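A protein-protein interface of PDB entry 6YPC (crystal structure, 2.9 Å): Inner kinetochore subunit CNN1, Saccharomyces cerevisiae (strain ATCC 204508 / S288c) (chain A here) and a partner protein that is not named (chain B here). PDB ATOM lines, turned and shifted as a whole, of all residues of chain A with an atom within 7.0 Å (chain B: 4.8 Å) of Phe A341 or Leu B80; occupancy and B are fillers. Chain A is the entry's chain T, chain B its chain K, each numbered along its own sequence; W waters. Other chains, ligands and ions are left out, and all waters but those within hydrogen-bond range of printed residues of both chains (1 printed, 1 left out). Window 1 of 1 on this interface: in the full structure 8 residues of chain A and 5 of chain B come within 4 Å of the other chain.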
ATOM      1  N   ILE A 334     -24.483   6.583   6.866  1.00  0.00           N
ATOM      2  CA  ILE A 334     -23.789   7.630   7.595  1.00  0.00           C
ATOM      3  C   ILE A 334     -24.700   8.848   7.653  1.00  0.00           C
ATOM      4  O   ILE A 334     -25.771   8.886   7.046  1.00  0.00           O
ATOM      5  CB  ILE A 334     -22.451   7.991   6.926  1.00  0.00           C
ATOM      6  CG1 ILE A 334     -22.682   8.219   5.433  1.00  0.00           C
ATOM      7  CG2 ILE A 334     -21.430   6.891   7.148  1.00  0.00           C
ATOM      8  CD1 ILE A 334     -21.428   8.459   4.647  1.00  0.00           C
ATOM      9  N   ASN A 336     -23.021  12.221   7.705  1.00  0.00           N
ATOM     10  CA  ASN A 336     -22.173  13.308   7.235  1.00  0.00           C
ATOM     11  C   ASN A 336     -20.873  12.684   6.752  1.00  0.00           C
ATOM     12  O   ASN A 336     -20.759  11.456   6.648  1.00  0.00           O
ATOM     13  CB  ASN A 336     -21.942  14.330   8.348  1.00  0.00           C
ATOM     14  CG  ASN A 336     -21.615  13.671   9.665  1.00  0.00           C
ATOM     15  OD1 ASN A 336     -21.819  12.465   9.830  1.00  0.00           O
ATOM     16  ND2 ASN A 336     -21.134  14.456  10.626  1.00  0.00           N
ATOM     17  N   VAL A 337     -19.885  13.526   6.464  1.00  0.00           N
ATOM     18  CA  VAL A 337     -18.615  13.003   5.976  1.00  0.00           C
ATOM     19  C   VAL A 337     -17.668  12.673   7.138  1.00  0.00           C
ATOM     20  O   VAL A 337     -16.757  11.848   6.996  1.00  0.00           O
ATOM     21  CB  VAL A 337     -17.984  14.012   5.006  1.00  0.00           C
ATOM     22  CG1 VAL A 337     -17.820  15.339   5.677  1.00  0.00           C
ATOM     23  CG2 VAL A 337     -16.660  13.527   4.458  1.00  0.00           C
ATOM     24  N   ASP A 338     -17.855  13.300   8.299  1.00  0.00           N
ATOM     25  CA  ASP A 338     -17.108  12.885   9.475  1.00  0.00           C
ATOM     26  C   ASP A 338     -17.315  11.408   9.762  1.00  0.00           C
ATOM     27  O   ASP A 338     -16.372  10.714  10.135  1.00  0.00           O
ATOM     28  CB  ASP A 338     -17.507  13.724  10.678  1.00  0.00           C
ATOM     29  CG  ASP A 338     -17.081  15.167  10.534  1.00  0.00           C
ATOM     30  OD1 ASP A 338     -15.938  15.404  10.067  1.00  0.00           O
ATOM     31  OD2 ASP A 338     -17.878  16.070  10.903  1.00  0.00           O
ATOM     32  N   ASP A 339     -18.537  10.904   9.588  1.00  0.00           N
ATOM     33  CA  ASP A 339     -18.774   9.471   9.767  1.00  0.00           C
ATOM     34  C   ASP A 339     -18.007   8.650   8.741  1.00  0.00           C
ATOM     35  O   ASP A 339     -17.551   7.540   9.043  1.00  0.00           O
ATOM     36  CB  ASP A 339     -20.271   9.148   9.674  1.00  0.00           C
ATOM     37  CG  ASP A 339     -21.049   9.542  10.934  1.00  0.00           C
ATOM     38  OD1 ASP A 339     -20.442  10.134  11.863  1.00  0.00           O
ATOM     39  OD2 ASP A 339     -22.273   9.243  10.990  1.00  0.00           O
ATOM     40  N   MET A 340     -17.847   9.173   7.529  1.00  0.00           N
ATOM     41  CA  MET A 340     -17.130   8.413   6.515  1.00  0.00           C
ATOM     42  C   MET A 340     -15.669   8.257   6.892  1.00  0.00           C
ATOM     43  O   MET A 340     -15.043   7.240   6.580  1.00  0.00           O
ATOM     44  CB  MET A 340     -17.256   9.089   5.151  1.00  0.00           C
ATOM     45  CG  MET A 340     -16.524   8.358   4.037  1.00  0.00           C
ATOM     46  SD  MET A 340     -17.196   6.711   3.700  1.00  0.00           S
ATOM     47  CE  MET A 340     -18.570   7.175   2.664  1.00  0.00           C
ATOM     48  N   PHE A 341     -15.107   9.257   7.560  1.00  0.00           N
ATOM     49  CA  PHE A 341     -13.713   9.159   7.961  1.00  0.00           C
ATOM     50  C   PHE A 341     -13.545   8.154   9.093  1.00  0.00           C
ATOM     51  O   PHE A 341     -12.649   7.302   9.057  1.00  0.00           O
ATOM     52  CB  PHE A 341     -13.189  10.525   8.362  1.00  0.00           C
ATOM     53  CG  PHE A 341     -11.768  10.501   8.790  1.00  0.00           C
ATOM     54  CD1 PHE A 341     -10.744  10.483   7.847  1.00  0.00           C
ATOM     55  CD2 PHE A 341     -11.444  10.467  10.134  1.00  0.00           C
ATOM     56  CE1 PHE A 341      -9.417  10.463   8.238  1.00  0.00           C
ATOM     57  CE2 PHE A 341     -10.131  10.449  10.533  1.00  0.00           C
ATOM     58  CZ  PHE A 341      -9.112  10.446   9.582  1.00  0.00           C
ATOM     59  N   GLU A 342     -14.413   8.227  10.099  1.00  0.00           N
ATOM     60  CA  GLU A 342     -14.521   7.148  11.066  1.00  0.00           C
ATOM     61  C   GLU A 342     -14.666   5.778  10.416  1.00  0.00           C
ATOM     62  O   GLU A 342     -14.328   4.772  11.049  1.00  0.00           O
ATOM     63  CB  GLU A 342     -15.700   7.401  11.986  1.00  0.00           C
ATOM     64  CG  GLU A 342     -15.663   8.762  12.649  1.00  0.00           C
ATOM     65  CD  GLU A 342     -14.676   8.822  13.817  1.00  0.00           C
ATOM     66  OE1 GLU A 342     -14.233   7.735  14.285  1.00  0.00           O
ATOM     67  OE2 GLU A 342     -14.369   9.958  14.270  1.00  0.00           O
ATOM     68  N   LEU A 343     -15.167   5.697   9.183  1.00  0.00           N
ATOM     69  CA  LEU A 343     -15.168   4.413   8.491  1.00  0.00           C
ATOM     70  C   LEU A 343     -13.829   4.142   7.834  1.00  0.00           C
ATOM     71  O   LEU A 343     -13.370   2.993   7.798  1.00  0.00           O
ATOM     72  CB  LEU A 343     -16.253   4.374   7.421  1.00  0.00           C
ATOM     73  CG  LEU A 343     -17.548   3.664   7.736  1.00  0.00           C
ATOM     74  CD1 LEU A 343     -18.023   4.087   9.115  1.00  0.00           C
ATOM     75  CD2 LEU A 343     -18.546   4.078   6.682  1.00  0.00           C
ATOM     76  N   ALA A 344     -13.232   5.181   7.251  1.00  0.00           N
ATOM     77  CA  ALA A 344     -11.896   5.047   6.698  1.00  0.00           C
ATOM     78  C   ALA A 344     -10.938   4.551   7.759  1.00  0.00           C
ATOM     79  O   ALA A 344     -10.170   3.611   7.533  1.00  0.00           O
ATOM     80  CB  ALA A 344     -11.430   6.389   6.139  1.00  0.00           C
ATOM     81  N   HIS A 345     -11.014   5.151   8.946  1.00  0.00           N
ATOM     82  CA  HIS A 345     -10.124   4.803  10.041  1.00  0.00           C
ATOM     83  C   HIS A 345     -10.243   3.344  10.428  1.00  0.00           C
ATOM     84  O   HIS A 345      -9.273   2.746  10.902  1.00  0.00           O
ATOM     85  CB  HIS A 345     -10.426   5.667  11.257  1.00  0.00           C
ATOM     86  CG  HIS A 345      -9.596   5.307  12.444  1.00  0.00           C
ATOM     87  ND1 HIS A 345     -10.133   4.786  13.602  1.00  0.00           N
ATOM     88  CD2 HIS A 345      -8.254   5.355  12.635  1.00  0.00           C
ATOM     89  CE1 HIS A 345      -9.162   4.549  14.466  1.00  0.00           C
ATOM     90  NE2 HIS A 345      -8.011   4.886  13.905  1.00  0.00           N
ATOM     91  N   GLU A 346     -11.414   2.752  10.253  1.00  0.00           N
ATOM     92  CA  GLU A 346     -11.592   1.389  10.710  1.00  0.00           C
ATOM     93  C   GLU A 346     -11.477   0.355   9.610  1.00  0.00           C
ATOM     94  O   GLU A 346     -11.432  -0.842   9.916  1.00  0.00           O
ATOM     95  CB  GLU A 346     -12.928   1.220  11.446  1.00  0.00           C
ATOM     96  CG  GLU A 346     -12.746   1.632  12.898  1.00  0.00           C
ATOM     97  CD  GLU A 346     -11.884   0.608  13.680  1.00  0.00           C
ATOM     98  OE1 GLU A 346     -10.895   1.066  14.311  1.00  0.00           O
ATOM     99  OE2 GLU A 346     -12.177  -0.625  13.666  1.00  0.00           O
ATOM    100  N   LEU A 347     -11.407   0.777   8.351  1.00  0.00           N
ATOM    101  CA  LEU A 347     -11.328  -0.158   7.242  1.00  0.00           C
ATOM    102  C   LEU A 347     -10.087   0.018   6.390  1.00  0.00           C
ATOM    103  O   LEU A 347      -9.708  -0.925   5.697  1.00  0.00           O
ATOM    104  CB  LEU A 347     -12.561  -0.033   6.333  1.00  0.00           C
ATOM    105  CG  LEU A 347     -13.950  -0.122   6.969  1.00  0.00           C
ATOM    106  CD1 LEU A 347     -14.993  -0.232   5.884  1.00  0.00           C
ATOM    107  CD2 LEU A 347     -14.072  -1.296   7.931  1.00  0.00           C
ATOM    108  N   LEU A 350      -3.162   2.588   7.543  1.00  0.00           N
ATOM    109  CA  LEU A 350      -2.786   3.924   7.980  1.00  0.00           C
ATOM    110  C   LEU A 350      -2.687   4.909   6.826  1.00  0.00           C
ATOM    111  O   LEU A 350      -3.396   5.919   6.792  1.00  0.00           O
ATOM    112  CB  LEU A 350      -1.453   3.865   8.730  1.00  0.00           C
ATOM    113  CG  LEU A 350      -1.243   5.057   9.657  1.00  0.00           C
ATOM    114  CD1 LEU A 350      -2.385   5.049  10.641  1.00  0.00           C
ATOM    115  CD2 LEU A 350       0.095   4.966  10.375  1.00  0.00           C
ATOM    116  N   LEU A 352      -3.457   5.031   3.660  1.00  0.00           N
ATOM    117  CA  LEU A 352      -4.650   5.418   2.931  1.00  0.00           C
ATOM    118  C   LEU A 352      -5.533   6.323   3.763  1.00  0.00           C
ATOM    119  O   LEU A 352      -6.271   7.137   3.206  1.00  0.00           O
ATOM    120  CB  LEU A 352      -5.410   4.183   2.486  1.00  0.00           C
ATOM    121  CG  LEU A 352      -4.636   3.555   1.332  1.00  0.00           C
ATOM    122  CD1 LEU A 352      -5.313   2.278   0.832  1.00  0.00           C
ATOM    123  CD2 LEU A 352      -4.469   4.582   0.209  1.00  0.00           C
ATOM    124  N   GLN A 353      -5.477   6.207   5.089  1.00  0.00           N
ATOM    125  CA  GLN A 353      -6.282   7.092   5.921  1.00  0.00           C
ATOM    126  C   GLN A 353      -5.857   8.531   5.722  1.00  0.00           C
ATOM    127  O   GLN A 353      -6.694   9.405   5.466  1.00  0.00           O
ATOM    128  CB  GLN A 353      -6.183   6.698   7.388  1.00  0.00           C
ATOM    129  CG  GLN A 353      -6.772   5.351   7.657  1.00  0.00           C
ATOM    130  CD  GLN A 353      -6.604   4.925   9.088  1.00  0.00           C
ATOM    131  OE1 GLN A 353      -6.280   5.734   9.953  1.00  0.00           O
ATOM    132  NE2 GLN A 353      -6.834   3.643   9.353  1.00  0.00           N
ATOM    133  N   SER A 354      -4.551   8.797   5.800  1.00  0.00           N
ATOM    134  CA  SER A 354      -4.078  10.147   5.529  1.00  0.00           C
ATOM    135  C   SER A 354      -4.496  10.609   4.133  1.00  0.00           C
ATOM    136  O   SER A 354      -4.855  11.774   3.955  1.00  0.00           O
ATOM    137  CB  SER A 354      -2.557  10.228   5.708  1.00  0.00           C
ATOM    138  OG  SER A 354      -2.126   9.626   6.932  1.00  0.00           O
ATOM    139  N   ILE A 356      -7.345   9.603   2.074  1.00  0.00           N
ATOM    140  CA  ILE A 356      -8.780   9.863   2.143  1.00  0.00           C
ATOM    141  C   ILE A 356      -9.094  11.114   2.944  1.00  0.00           C
ATOM    142  O   ILE A 356     -10.020  11.859   2.607  1.00  0.00           O
ATOM    143  CB  ILE A 356      -9.489   8.635   2.734  1.00  0.00           C
ATOM    144  CG1 ILE A 356      -9.476   7.500   1.732  1.00  0.00           C
ATOM    145  CG2 ILE A 356     -10.921   8.955   3.069  1.00  0.00           C
ATOM    146  CD1 ILE A 356     -10.583   7.586   0.719  1.00  0.00           C
ATOM    147  N   GLU A 357      -8.338  11.375   4.013  1.00  0.00           N
ATOM    148  CA  GLU A 357      -8.596  12.571   4.807  1.00  0.00           C
ATOM    149  C   GLU A 357      -8.591  13.815   3.925  1.00  0.00           C
ATOM    150  O   GLU A 357      -9.535  14.617   3.962  1.00  0.00           O
ATOM    151  CB  GLU A 357      -7.575  12.699   5.944  1.00  0.00           C
ATOM    152  CG  GLU A 357      -8.101  13.542   7.116  1.00  0.00           C
ATOM    153  CD  GLU A 357      -7.019  14.032   8.097  1.00  0.00           C
ATOM    154  OE1 GLU A 357      -5.946  13.382   8.202  1.00  0.00           O
ATOM    155  OE2 GLU A 357      -7.242  15.097   8.744  1.00  0.00           O
ATOM    156  N   SER A 358      -7.564  13.961   3.076  1.00  0.00           N
ATOM    157  CA  SER A 358      -7.494  15.104   2.160  1.00  0.00           C
ATOM    158  C   SER A 358      -8.573  15.058   1.068  1.00  0.00           C
ATOM    159  O   SER A 358      -9.048  16.111   0.613  1.00  0.00           O
ATOM    160  CB  SER A 358      -6.124  15.175   1.499  1.00  0.00           C
ATOM    161  OG  SER A 358      -5.085  14.797   2.390  1.00  0.00           O
ATOM    162  N   LEU A 360     -11.493  14.486   1.552  1.00  0.00           N
ATOM    163  CA  LEU A 360     -12.735  14.978   2.148  1.00  0.00           C
ATOM    164  C   LEU A 360     -12.594  16.380   2.772  1.00  0.00           C
ATOM    165  O   LEU A 360     -11.941  16.579   3.810  1.00  0.00           O
ATOM    166  CB  LEU A 360     -13.229  13.973   3.186  1.00  0.00           C
ATOM    167  CG  LEU A 360     -13.094  12.518   2.731  1.00  0.00           C
ATOM    168  CD1 LEU A 360     -13.593  11.556   3.795  1.00  0.00           C
ATOM    169  CD2 LEU A 360     -13.848  12.308   1.445  1.00  0.00           C
ATOM    170  N   TYR B  76      -7.892  16.403  16.311  1.00  0.00           N
ATOM    171  CA  TYR B  76      -8.649  15.217  16.665  1.00  0.00           C
ATOM    172  C   TYR B  76      -8.417  14.118  15.648  1.00  0.00           C
ATOM    173  O   TYR B  76      -8.090  12.990  16.011  1.00  0.00           O
ATOM    174  CB  TYR B  76     -10.136  15.538  16.759  1.00  0.00           C
ATOM    175  CG  TYR B  76     -10.941  14.287  16.639  1.00  0.00           C
ATOM    176  CD1 TYR B  76     -10.992  13.376  17.686  1.00  0.00           C
ATOM    177  CD2 TYR B  76     -11.605  13.979  15.458  1.00  0.00           C
ATOM    178  CE1 TYR B  76     -11.703  12.203  17.573  1.00  0.00           C
ATOM    179  CE2 TYR B  76     -12.324  12.807  15.329  1.00  0.00           C
ATOM    180  CZ  TYR B  76     -12.375  11.922  16.389  1.00  0.00           C
ATOM    181  OH  TYR B  76     -13.088  10.749  16.259  1.00  0.00           O
ATOM    182  N   ARG B  77      -8.545  14.436  14.359  1.00  0.00           N
ATOM    183  CA  ARG B  77      -8.349  13.401  13.347  1.00  0.00           C
ATOM    184  C   ARG B  77      -6.928  12.865  13.356  1.00  0.00           C
ATOM    185  O   ARG B  77      -6.704  11.691  13.031  1.00  0.00           O
ATOM    186  CB  ARG B  77      -8.711  13.929  11.967  1.00  0.00           C
ATOM    187  CG  ARG B  77     -10.189  13.750  11.690  1.00  0.00           C
ATOM    188  CD  ARG B  77     -10.614  14.186  10.296  1.00  0.00           C
ATOM    189  NE  ARG B  77     -10.333  15.599  10.081  1.00  0.00           N
ATOM    190  CZ  ARG B  77     -11.270  16.533  10.002  1.00  0.00           C
ATOM    191  NH1 ARG B  77     -12.559  16.207  10.123  1.00  0.00           N
ATOM    192  NH2 ARG B  77     -10.910  17.794   9.803  1.00  0.00           N
ATOM    193  N   LEU B  78      -5.965  13.704  13.729  1.00  0.00           N
ATOM    194  CA  LEU B  78      -4.574  13.280  13.760  1.00  0.00           C
ATOM    195  C   LEU B  78      -4.347  12.295  14.895  1.00  0.00           C
ATOM    196  O   LEU B  78      -3.708  11.247  14.711  1.00  0.00           O
ATOM    197  CB  LEU B  78      -3.677  14.505  13.908  1.00  0.00           C
ATOM    198  CG  LEU B  78      -2.277  14.272  14.444  1.00  0.00           C
ATOM    199  CD1 LEU B  78      -1.436  13.703  13.337  1.00  0.00           C
ATOM    200  CD2 LEU B  78      -1.679  15.580  14.956  1.00  0.00           C
ATOM    201  N   LEU B  79      -4.878  12.615  16.079  1.00  0.00           N
ATOM    202  CA  LEU B  79      -4.833  11.678  17.195  1.00  0.00           C
ATOM    203  C   LEU B  79      -5.513  10.374  16.824  1.00  0.00           C
ATOM    204  O   LEU B  79      -4.983   9.286  17.078  1.00  0.00           O
ATOM    205  CB  LEU B  79      -5.495  12.297  18.423  1.00  0.00           C
ATOM    206  CG  LEU B  79      -4.935  13.683  18.739  1.00  0.00           C
ATOM    207  CD1 LEU B  79      -5.903  14.501  19.588  1.00  0.00           C
ATOM    208  CD2 LEU B  79      -3.602  13.521  19.415  1.00  0.00           C
ATOM    209  N   LEU B  80      -6.671  10.464  16.188  1.00  0.00           N
ATOM    210  CA  LEU B  80      -7.367   9.265  15.758  1.00  0.00           C
ATOM    211  C   LEU B  80      -6.471   8.398  14.871  1.00  0.00           C
ATOM    212  O   LEU B  80      -6.328   7.194  15.108  1.00  0.00           O
ATOM    213  CB  LEU B  80      -8.653   9.668  15.040  1.00  0.00           C
ATOM    214  CG  LEU B  80      -9.609   8.519  14.756  1.00  0.00           C
ATOM    215  CD1 LEU B  80     -10.083   7.972  16.061  1.00  0.00           C
ATOM    216  CD2 LEU B  80     -10.769   8.979  13.917  1.00  0.00           C
ATOM    217  N   ARG B  81      -5.835   9.001  13.860  1.00  0.00           N
ATOM    218  CA  ARG B  81      -5.029   8.220  12.925  1.00  0.00           C
ATOM    219  C   ARG B  81      -3.900   7.502  13.642  1.00  0.00           C
ATOM    220  O   ARG B  81      -3.676   6.300  13.425  1.00  0.00           O
ATOM    221  CB  ARG B  81      -4.460   9.117  11.827  1.00  0.00           C
ATOM    222  CG  ARG B  81      -5.240   9.058  10.536  1.00  0.00           C
ATOM    223  CD  ARG B  81      -4.615   9.906   9.476  1.00  0.00           C
ATOM    224  NE  ARG B  81      -4.512  11.277   9.936  1.00  0.00           N
ATOM    225  CZ  ARG B  81      -3.360  11.910  10.111  1.00  0.00           C
ATOM    226  NH1 ARG B  81      -2.215  11.280   9.846  1.00  0.00           N
ATOM    227  NH2 ARG B  81      -3.359  13.168  10.551  1.00  0.00           N
ATOM    228  N   ALA B  82      -3.187   8.234  14.511  1.00  0.00           N
ATOM    229  CA  ALA B  82      -2.073   7.719  15.307  1.00  0.00           C
ATOM    230  C   ALA B  82      -2.493   6.649  16.307  1.00  0.00           C
ATOM    231  O   ALA B  82      -1.618   6.003  16.895  1.00  0.00           O
ATOM    232  CB  ALA B  82      -1.389   8.867  16.055  1.00  0.00           C
ATOM    233  N   ASN B  83      -3.792   6.455  16.522  1.00  0.00           N
ATOM    234  CA  ASN B  83      -4.271   5.392  17.388  1.00  0.00           C
ATOM    235  C   ASN B  83      -3.815   5.608  18.815  1.00  0.00           C
ATOM    236  O   ASN B  83      -3.392   4.663  19.473  1.00  0.00           O
ATOM    237  CB  ASN B  83      -3.797   4.017  16.909  1.00  0.00           C
ATOM    238  CG  ASN B  83      -4.496   3.569  15.663  1.00  0.00           C
ATOM    239  OD1 ASN B  83      -5.716   3.737  15.528  1.00  0.00           O
ATOM    240  ND2 ASN B  83      -3.742   2.964  14.746  1.00  0.00           N
ATOM    241  N   ILE B  85      -5.714   7.708  21.077  1.00  0.00           N
ATOM    242  CA  ILE B  85      -6.838   8.152  21.889  1.00  0.00           C
ATOM    243  C   ILE B  85      -7.947   7.116  21.804  1.00  0.00           C
ATOM    244  O   ILE B  85      -8.054   6.361  20.831  1.00  0.00           O
ATOM    245  CB  ILE B  85      -7.384   9.522  21.452  1.00  0.00           C
ATOM    246  CG1 ILE B  85      -7.708   9.514  19.966  1.00  0.00           C
ATOM    247  CG2 ILE B  85      -6.419  10.626  21.799  1.00  0.00           C
ATOM    248  CD1 ILE B  85      -8.599  10.665  19.582  1.00  0.00           C
ATOM    249  N   VAL B  87     -12.166   6.883  22.042  1.00  0.00           N
ATOM    250  CA  VAL B  87     -13.372   7.702  21.983  1.00  0.00           C
ATOM    251  C   VAL B  87     -14.574   6.831  22.358  1.00  0.00           C
ATOM    252  O   VAL B  87     -14.855   5.827  21.694  1.00  0.00           O
ATOM    253  CB  VAL B  87     -13.545   8.360  20.603  1.00  0.00           C
ATOM    254  CG1 VAL B  87     -14.454   9.561  20.689  1.00  0.00           C
ATOM    255  CG2 VAL B  87     -12.229   8.811  20.090  1.00  0.00           C
HETATM  256  O   HOH W   1     -12.699  15.589   6.753  1.00  0.00           O
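NE of Arg B77 lies within salt-bridge range of OE2 of Glu A357. The side-chain carboxylate (OE2) of Glu A342 sits at hydrogen-bond distance from the side-chain hydroxyl (OH) of Tyr B76, at 2.5 Å. O of Leu B80 is in hydrogen-bond range of NE2 of His A345 (3.1 Å). The guanidinium group (NH1) of Arg B77 is in salt-bridge range of the side-chain carboxylate (OD1) of Asp A338 (3.5 Å). The guanidinium group (NH1) of Arg B81 lies within hydrogen-bond range of the side-chain hydroxyl (OG) of Ser A354, at 3.4 Å. The side-chain carboxylate (OE1) of Glu A357 is in salt-bridge range of the guanidinium group (NE) of Arg B81, 3.1 Å away. NE2 of His A345 lies within hydrogen-bond range of OD1 of Asn B83 (3.0 Å).
O of Ser A354 sits at hydrogen-bond distance from OG of Ser A358 (3.4 Å). The backbone carbonyl oxygen (O) of His A345 sits at hydrogen-bond distance from the side-chain amide nitrogen (NE2) of Gln A353 (3.0 Å).
Among the printed residues, merely in contact across the chains: Phe A341 with Arg B77 (3.5 Å), Phe A341 with Leu B80 (3.7 Å), Glu A342 with Leu B80 (3.7 Å), Leu A350 with Arg B81 (3.3 Å) and Gln A353 with Arg B81 (3.5 Å).
Of chain B, only Arg B77 (3.5 Å) and Leu B80 (3.7 Å) come within 4 Å of Phe A341. Leu B80 touches just these residues of chain A: Phe A341, Glu A342 and His A345. Of the printed residues of chain B, Glu A342 touches Tyr B76 (2.5 Å) and Leu B80 (3.7 Å). Of the printed residues of chain B, His A345 touches Leu B80 (3.1 Å) and Asn B83 (3.0 Å). Printed residues of chain B within 4 Å of Gln A353: Arg B81. Of the printed residues of chain B, Asp A338 touches Arg B77. The nearest printed residue of chain B that does not touch Gln A353 is Leu B80 (5.4 Å).
Of the 21 printed residues of chain A, 8 touch a printed residue of chain B. Printed residues of chain A that touch a printed residue of chain B: Asp A338, Phe A341, Glu A342, His A345, Leu A350, Gln A353, Ser A354 and Glu A357. Among the printed residues, 12 pairs touch across the chains. Among the printed residues, Asp or Glu carboxylates within 4 Å of a Lys or Arg side-chain nitrogen of the other chain: Asp A338 with Arg B77, Glu A357 with Arg B77 and Glu A357 with Arg B81.
Water W1 lies within hydrogen-bond range of O of Leu A360 (3.2 Å) and NH1 of Arg B77 (3.4 Å).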
